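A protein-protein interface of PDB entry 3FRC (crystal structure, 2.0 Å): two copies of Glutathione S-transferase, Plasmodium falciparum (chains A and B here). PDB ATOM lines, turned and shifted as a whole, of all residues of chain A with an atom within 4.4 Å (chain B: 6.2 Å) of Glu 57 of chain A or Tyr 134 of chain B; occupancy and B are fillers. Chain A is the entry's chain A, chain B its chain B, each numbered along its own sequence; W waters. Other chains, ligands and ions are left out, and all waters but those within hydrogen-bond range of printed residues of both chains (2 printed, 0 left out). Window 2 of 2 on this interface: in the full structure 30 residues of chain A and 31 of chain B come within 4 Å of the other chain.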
ATOM      1  N   PHE A  45     -35.217  -8.978   2.344  1.00  0.00           N
ATOM      2  CA  PHE A  45     -33.858  -9.436   2.655  1.00  0.00           C
ATOM      3  C   PHE A  45     -33.020  -9.661   1.389  1.00  0.00           C
ATOM      4  O   PHE A  45     -31.812  -9.445   1.386  1.00  0.00           O
ATOM      5  CB  PHE A  45     -33.901 -10.714   3.504  1.00  0.00           C
ATOM      6  CG  PHE A  45     -32.545 -11.203   3.946  1.00  0.00           C
ATOM      7  CD1 PHE A  45     -31.688 -10.375   4.671  1.00  0.00           C
ATOM      8  CD2 PHE A  45     -32.132 -12.500   3.655  1.00  0.00           C
ATOM      9  CE1 PHE A  45     -30.438 -10.823   5.085  1.00  0.00           C
ATOM     10  CE2 PHE A  45     -30.881 -12.959   4.070  1.00  0.00           C
ATOM     11  CZ  PHE A  45     -30.036 -12.115   4.785  1.00  0.00           C
ATOM     12  N   LYS A  49     -29.599  -7.272   0.574  1.00  0.00           N
ATOM     13  CA  LYS A  49     -28.285  -7.831   0.255  1.00  0.00           C
ATOM     14  C   LYS A  49     -27.683  -7.248  -1.024  1.00  0.00           C
ATOM     15  O   LYS A  49     -26.473  -7.015  -1.090  1.00  0.00           O
ATOM     16  CB  LYS A  49     -28.356  -9.360   0.174  1.00  0.00           C
ATOM     17  CG  LYS A  49     -28.531 -10.046   1.534  1.00  0.00           C
ATOM     18  CD  LYS A  49     -28.369 -11.557   1.440  1.00  0.00           C
ATOM     19  CE  LYS A  49     -29.586 -12.238   0.819  1.00  0.00           C
ATOM     20  NZ  LYS A  49     -29.382 -13.716   0.722  1.00  0.00           N
ATOM     21  N   THR A  54     -22.693  -6.263   2.550  1.00  0.00           N
ATOM     22  CA  THR A  54     -22.506  -7.033   3.785  1.00  0.00           C
ATOM     23  C   THR A  54     -21.371  -8.019   3.566  1.00  0.00           C
ATOM     24  O   THR A  54     -21.193  -8.511   2.452  1.00  0.00           O
ATOM     25  CB  THR A  54     -23.783  -7.810   4.194  1.00  0.00           C
ATOM     26  OG1 THR A  54     -24.031  -8.859   3.252  1.00  0.00           O
ATOM     27  CG2 THR A  54     -24.993  -6.877   4.266  1.00  0.00           C
ATOM     28  N   PRO A  55     -20.576  -8.292   4.618  1.00  0.00           N
ATOM     29  CA  PRO A  55     -19.443  -9.203   4.432  1.00  0.00           C
ATOM     30  C   PRO A  55     -19.834 -10.679   4.272  1.00  0.00           C
ATOM     31  O   PRO A  55     -19.174 -11.406   3.522  1.00  0.00           O
ATOM     32  CB  PRO A  55     -18.600  -8.989   5.697  1.00  0.00           C
ATOM     33  CG  PRO A  55     -19.550  -8.467   6.715  1.00  0.00           C
ATOM     34  CD  PRO A  55     -20.639  -7.740   5.987  1.00  0.00           C
ATOM     35  N   PHE A  56     -20.900 -11.105   4.947  1.00  0.00           N
ATOM     36  CA  PHE A  56     -21.282 -12.514   4.982  1.00  0.00           C
ATOM     37  C   PHE A  56     -22.751 -12.783   4.614  1.00  0.00           C
ATOM     38  O   PHE A  56     -23.261 -13.872   4.865  1.00  0.00           O
ATOM     39  CB  PHE A  56     -20.982 -13.114   6.365  1.00  0.00           C
ATOM     40  CG  PHE A  56     -19.612 -12.783   6.897  1.00  0.00           C
ATOM     41  CD1 PHE A  56     -19.472 -12.015   8.042  1.00  0.00           C
ATOM     42  CD2 PHE A  56     -18.461 -13.261   6.268  1.00  0.00           C
ATOM     43  CE1 PHE A  56     -18.210 -11.718   8.555  1.00  0.00           C
ATOM     44  CE2 PHE A  56     -17.190 -12.961   6.772  1.00  0.00           C
ATOM     45  CZ  PHE A  56     -17.071 -12.187   7.922  1.00  0.00           C
ATOM     46  N   GLU A  57     -23.422 -11.791   4.029  1.00  0.00           N
ATOM     47  CA  GLU A  57     -24.842 -11.894   3.651  1.00  0.00           C
ATOM     48  C   GLU A  57     -25.750 -12.308   4.811  1.00  0.00           C
ATOM     49  O   GLU A  57     -26.761 -12.999   4.622  1.00  0.00           O
ATOM     50  CB  GLU A  57     -25.022 -12.807   2.436  1.00  0.00           C
ATOM     51  CG  GLU A  57     -24.319 -12.275   1.194  1.00  0.00           C
ATOM     52  CD  GLU A  57     -24.377 -13.229   0.021  1.00  0.00           C
ATOM     53  OE1 GLU A  57     -24.496 -14.456   0.232  1.00  0.00           O
ATOM     54  OE2 GLU A  57     -24.297 -12.744  -1.125  1.00  0.00           O
ATOM     55  N   GLN A  58     -25.370 -11.871   6.012  1.00  0.00           N
ATOM     56  CA  GLN A  58     -26.119 -12.132   7.230  1.00  0.00           C
ATOM     57  C   GLN A  58     -26.560 -10.810   7.854  1.00  0.00           C
ATOM     58  O   GLN A  58     -25.953  -9.755   7.618  1.00  0.00           O
ATOM     59  CB  GLN A  58     -25.249 -12.869   8.258  1.00  0.00           C
ATOM     60  CG  GLN A  58     -24.807 -14.283   7.892  1.00  0.00           C
ATOM     61  CD  GLN A  58     -23.779 -14.842   8.885  1.00  0.00           C
ATOM     62  OE1 GLN A  58     -22.960 -14.096   9.445  1.00  0.00           O
ATOM     63  NE2 GLN A  58     -23.824 -16.157   9.108  1.00  0.00           N
ATOM     64  N   PRO B 129     -18.015 -23.180  -0.445  1.00  0.00           N
ATOM     65  CA  PRO B 129     -17.699 -22.291  -1.571  1.00  0.00           C
ATOM     66  C   PRO B 129     -18.142 -20.855  -1.311  1.00  0.00           C
ATOM     67  O   PRO B 129     -17.427 -19.915  -1.648  1.00  0.00           O
ATOM     68  CB  PRO B 129     -18.508 -22.891  -2.730  1.00  0.00           C
ATOM     69  CG  PRO B 129     -18.796 -24.293  -2.318  1.00  0.00           C
ATOM     70  CD  PRO B 129     -18.976 -24.227  -0.840  1.00  0.00           C
ATOM     71  N   LYS B 130     -19.316 -20.715  -0.706  1.00  0.00           N
ATOM     72  CA  LYS B 130     -19.940 -19.421  -0.434  1.00  0.00           C
ATOM     73  C   LYS B 130     -19.126 -18.609   0.577  1.00  0.00           C
ATOM     74  O   LYS B 130     -18.867 -17.416   0.375  1.00  0.00           O
ATOM     75  CB  LYS B 130     -21.349 -19.671   0.092  1.00  0.00           C
ATOM     76  CG  LYS B 130     -22.203 -18.446   0.308  1.00  0.00           C
ATOM     77  CD  LYS B 130     -23.600 -18.852   0.716  1.00  0.00           C
ATOM     78  CE  LYS B 130     -23.659 -19.241   2.174  1.00  0.00           C
ATOM     79  NZ  LYS B 130     -25.073 -19.396   2.618  1.00  0.00           N
ATOM     80  N   TRP B 131     -18.717 -19.263   1.656  1.00  0.00           N
ATOM     81  CA  TRP B 131     -17.896 -18.622   2.684  1.00  0.00           C
ATOM     82  C   TRP B 131     -16.472 -18.343   2.226  1.00  0.00           C
ATOM     83  O   TRP B 131     -15.891 -17.322   2.583  1.00  0.00           O
ATOM     84  CB  TRP B 131     -17.929 -19.438   3.977  1.00  0.00           C
ATOM     85  CG  TRP B 131     -19.172 -19.146   4.759  1.00  0.00           C
ATOM     86  CD1 TRP B 131     -20.392 -19.739   4.616  1.00  0.00           C
ATOM     87  CD2 TRP B 131     -19.321 -18.160   5.787  1.00  0.00           C
ATOM     88  NE1 TRP B 131     -21.296 -19.188   5.501  1.00  0.00           N
ATOM     89  CE2 TRP B 131     -20.661 -18.220   6.232  1.00  0.00           C
ATOM     90  CE3 TRP B 131     -18.450 -17.242   6.385  1.00  0.00           C
ATOM     91  CZ2 TRP B 131     -21.154 -17.385   7.241  1.00  0.00           C
ATOM     92  CZ3 TRP B 131     -18.943 -16.418   7.392  1.00  0.00           C
ATOM     93  CH2 TRP B 131     -20.281 -16.495   7.805  1.00  0.00           C
ATOM     94  N   SER B 132     -15.905 -19.243   1.426  1.00  0.00           N
ATOM     95  CA  SER B 132     -14.618 -18.969   0.786  1.00  0.00           C
ATOM     96  C   SER B 132     -14.681 -17.689  -0.056  1.00  0.00           C
ATOM     97  O   SER B 132     -13.752 -16.875  -0.026  1.00  0.00           O
ATOM     98  CB  SER B 132     -14.176 -20.161  -0.061  1.00  0.00           C
ATOM     99  OG  SER B 132     -14.024 -21.314   0.751  1.00  0.00           O
ATOM    100  N   GLY B 133     -15.788 -17.513  -0.783  1.00  0.00           N
ATOM    101  CA  GLY B 133     -16.067 -16.277  -1.527  1.00  0.00           C
ATOM    102  C   GLY B 133     -16.127 -15.019  -0.675  1.00  0.00           C
ATOM    103  O   GLY B 133     -15.632 -13.959  -1.079  1.00  0.00           O
ATOM    104  N   TYR B 134     -16.745 -15.122   0.500  1.00  0.00           N
ATOM    105  CA  TYR B 134     -16.798 -13.993   1.435  1.00  0.00           C
ATOM    106  C   TYR B 134     -15.400 -13.571   1.874  1.00  0.00           C
ATOM    107  O   TYR B 134     -15.075 -12.380   1.878  1.00  0.00           O
ATOM    108  CB  TYR B 134     -17.623 -14.330   2.681  1.00  0.00           C
ATOM    109  CG  TYR B 134     -19.070 -14.711   2.454  1.00  0.00           C
ATOM    110  CD1 TYR B 134     -19.776 -14.263   1.333  1.00  0.00           C
ATOM    111  CD2 TYR B 134     -19.753 -15.485   3.402  1.00  0.00           C
ATOM    112  CE1 TYR B 134     -21.115 -14.612   1.144  1.00  0.00           C
ATOM    113  CE2 TYR B 134     -21.084 -15.838   3.219  1.00  0.00           C
ATOM    114  CZ  TYR B 134     -21.756 -15.393   2.092  1.00  0.00           C
ATOM    115  OH  TYR B 134     -23.070 -15.743   1.917  1.00  0.00           O
ATOM    116  N   PHE B 135     -14.581 -14.546   2.258  1.00  0.00           N
ATOM    117  CA  PHE B 135     -13.205 -14.262   2.692  1.00  0.00           C
ATOM    118  C   PHE B 135     -12.332 -13.721   1.563  1.00  0.00           C
ATOM    119  O   PHE B 135     -11.561 -12.779   1.763  1.00  0.00           O
ATOM    120  CB  PHE B 135     -12.576 -15.489   3.369  1.00  0.00           C
ATOM    121  CG  PHE B 135     -13.236 -15.862   4.671  1.00  0.00           C
ATOM    122  CD1 PHE B 135     -13.759 -17.139   4.866  1.00  0.00           C
ATOM    123  CD2 PHE B 135     -13.348 -14.926   5.706  1.00  0.00           C
ATOM    124  CE1 PHE B 135     -14.388 -17.483   6.065  1.00  0.00           C
ATOM    125  CE2 PHE B 135     -13.970 -15.263   6.907  1.00  0.00           C
ATOM    126  CZ  PHE B 135     -14.486 -16.544   7.090  1.00  0.00           C
ATOM    127  N   GLU B 136     -12.478 -14.306   0.376  1.00  0.00           N
ATOM    128  CA  GLU B 136     -11.816 -13.811  -0.842  1.00  0.00           C
ATOM    129  C   GLU B 136     -12.108 -12.328  -1.096  1.00  0.00           C
ATOM    130  O   GLU B 136     -11.194 -11.555  -1.394  1.00  0.00           O
ATOM    131  CB  GLU B 136     -12.237 -14.660  -2.052  1.00  0.00           C
ATOM    132  CG  GLU B 136     -11.469 -14.393  -3.344  1.00  0.00           C
ATOM    133  CD  GLU B 136     -10.056 -14.969  -3.352  1.00  0.00           C
ATOM    134  OE1 GLU B 136      -9.696 -15.765  -2.456  1.00  0.00           O
ATOM    135  OE2 GLU B 136      -9.296 -14.618  -4.275  1.00  0.00           O
ATOM    136  N   LYS B 137     -13.376 -11.936  -0.963  1.00  0.00           N
ATOM    137  CA  LYS B 137     -13.794 -10.546  -1.177  1.00  0.00           C
ATOM    138  C   LYS B 137     -13.229  -9.602  -0.111  1.00  0.00           C
ATOM    139  O   LYS B 137     -12.830  -8.473  -0.409  1.00  0.00           O
ATOM    140  CB  LYS B 137     -15.324 -10.451  -1.251  1.00  0.00           C
ATOM    141  CG  LYS B 137     -15.835  -9.162  -1.883  1.00  0.00           C
ATOM    142  CD  LYS B 137     -17.117  -9.385  -2.685  1.00  0.00           C
ATOM    143  CE  LYS B 137     -18.368  -9.188  -1.843  1.00  0.00           C
ATOM    144  NZ  LYS B 137     -19.587  -9.045  -2.694  1.00  0.00           N
ATOM    145  N   LEU B 138     -13.167 -10.079   1.127  1.00  0.00           N
ATOM    146  CA  LEU B 138     -12.571  -9.307   2.210  1.00  0.00           C
ATOM    147  C   LEU B 138     -11.076  -9.056   2.002  1.00  0.00           C
ATOM    148  O   LEU B 138     -10.573  -7.970   2.306  1.00  0.00           O
ATOM    149  CB  LEU B 138     -12.820  -9.985   3.562  1.00  0.00           C
ATOM    150  CG  LEU B 138     -14.239  -9.880   4.130  1.00  0.00           C
ATOM    151  CD1 LEU B 138     -14.427 -10.897   5.251  1.00  0.00           C
ATOM    152  CD2 LEU B 138     -14.558  -8.461   4.629  1.00  0.00           C
ATOM    153  N   LEU B 139     -10.375 -10.059   1.483  1.00  0.00           N
ATOM    154  CA  LEU B 139      -8.954  -9.913   1.175  1.00  0.00           C
ATOM    155  C   LEU B 139      -8.720  -8.938   0.035  1.00  0.00           C
ATOM    156  O   LEU B 139      -7.815  -8.115   0.107  1.00  0.00           O
ATOM    157  CB  LEU B 139      -8.331 -11.258   0.826  1.00  0.00           C
ATOM    158  CG  LEU B 139      -7.864 -12.139   1.972  1.00  0.00           C
ATOM    159  CD1 LEU B 139      -7.603 -13.517   1.437  1.00  0.00           C
ATOM    160  CD2 LEU B 139      -6.606 -11.568   2.625  1.00  0.00           C
ATOM    161  N   PHE B 153      -6.018  -9.515   6.291  1.00  0.00           N
ATOM    162  CA  PHE B 153      -7.450  -9.248   6.301  1.00  0.00           C
ATOM    163  C   PHE B 153      -7.749  -7.863   6.860  1.00  0.00           C
ATOM    164  O   PHE B 153      -8.706  -7.209   6.436  1.00  0.00           O
ATOM    165  CB  PHE B 153      -8.198 -10.307   7.121  1.00  0.00           C
ATOM    166  CG  PHE B 153      -8.570 -11.515   6.330  1.00  0.00           C
ATOM    167  CD1 PHE B 153      -7.735 -12.625   6.305  1.00  0.00           C
ATOM    168  CD2 PHE B 153      -9.751 -11.539   5.590  1.00  0.00           C
ATOM    169  CE1 PHE B 153      -8.071 -13.754   5.552  1.00  0.00           C
ATOM    170  CE2 PHE B 153     -10.101 -12.658   4.842  1.00  0.00           C
ATOM    171  CZ  PHE B 153      -9.253 -13.770   4.818  1.00  0.00           C
HETATM  172  O   HOH W   1     -17.201 -10.633   1.962  1.00  0.00           O
HETATM  173  O   HOH W   2     -24.280 -16.163   4.442  1.00  0.00           O
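The backbone NH (N) of Glu 57 of chain A lies within hydrogen-bond range of the side-chain hydroxyl (OG1) of Thr 54 of chain A (3.1 Å).
Water W2 bridges O of Phe 56 of chain A and OH of Tyr 134 of chain B. Water W1 lies within hydrogen-bond range of the backbone carbonyl oxygen (O) of Pro 55 of chain A (2.6 Å) and the backbone carbonyl oxygen (O) of Tyr 134 of chain B (2.8 Å).
No position is printed for both chains. Of the 7 pairs that touch across the chains among the printed residues, none has its exchanged pair printed and touching as well.
Among the printed residues, pairs that only touch across the chains: Pro 55 of chain A with Tyr 134 of chain B, Phe 56 of chain A with Trp 131 of chain B, Phe 56 of chain A with Phe 135 of chain B, Phe 56 of chain A with Leu 138 of chain B and Gln 58 of chain A with Trp 131 of chain B.
OH of Tyr 134 of chain B sits close to O of Phe 56 of chain A, at 3.5 Å. The side-chain hydroxyl (OH) of Tyr 134 of chain B sits at hydrogen-bond distance from the side-chain carboxylate (OE1) of Glu 57 of chain A, 2.6 Å away.
Printed residues of chain B within 4 Å of Pro 55 of chain A: Tyr 134. Printed residues of chain B within 4 Å of Phe 56 of chain A: Trp 131, Tyr 134, Phe 135 and Leu 138. Of chain B, only Tyr 134 comes within 4 Å of Glu 57 of chain A. Of the printed residues of chain A, Trp 131 of chain B touches Phe 56 (3.4 Å) and Gln 58 (3.5 Å). Printed residues of chain A within 4 Å of Tyr 134 of chain B: Pro 55, Phe 56 and Glu 57. Printed residues of chain A within 4 Å of Phe 135 of chain B: Phe 56. The nearest residue of chain B that does not touch Glu 57 of chain A is Lys 130 of chain B (4.5 Å). The nearest printed residue of chain A that does not touch Tyr 134 of chain B is Thr 54 of chain A (6.0 Å).
Of the 7 printed residues of chain A, 4 touch a printed residue of chain B. Hydrophobic or aromatic side chains of chain B that line the printed part of chain A: Trp 131, Tyr 134, Phe 135 and Leu 138. Among the printed residues, no Asp or Glu carboxylate lies within 4 Å of a Lys or Arg side-chain nitrogen of the other chain.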
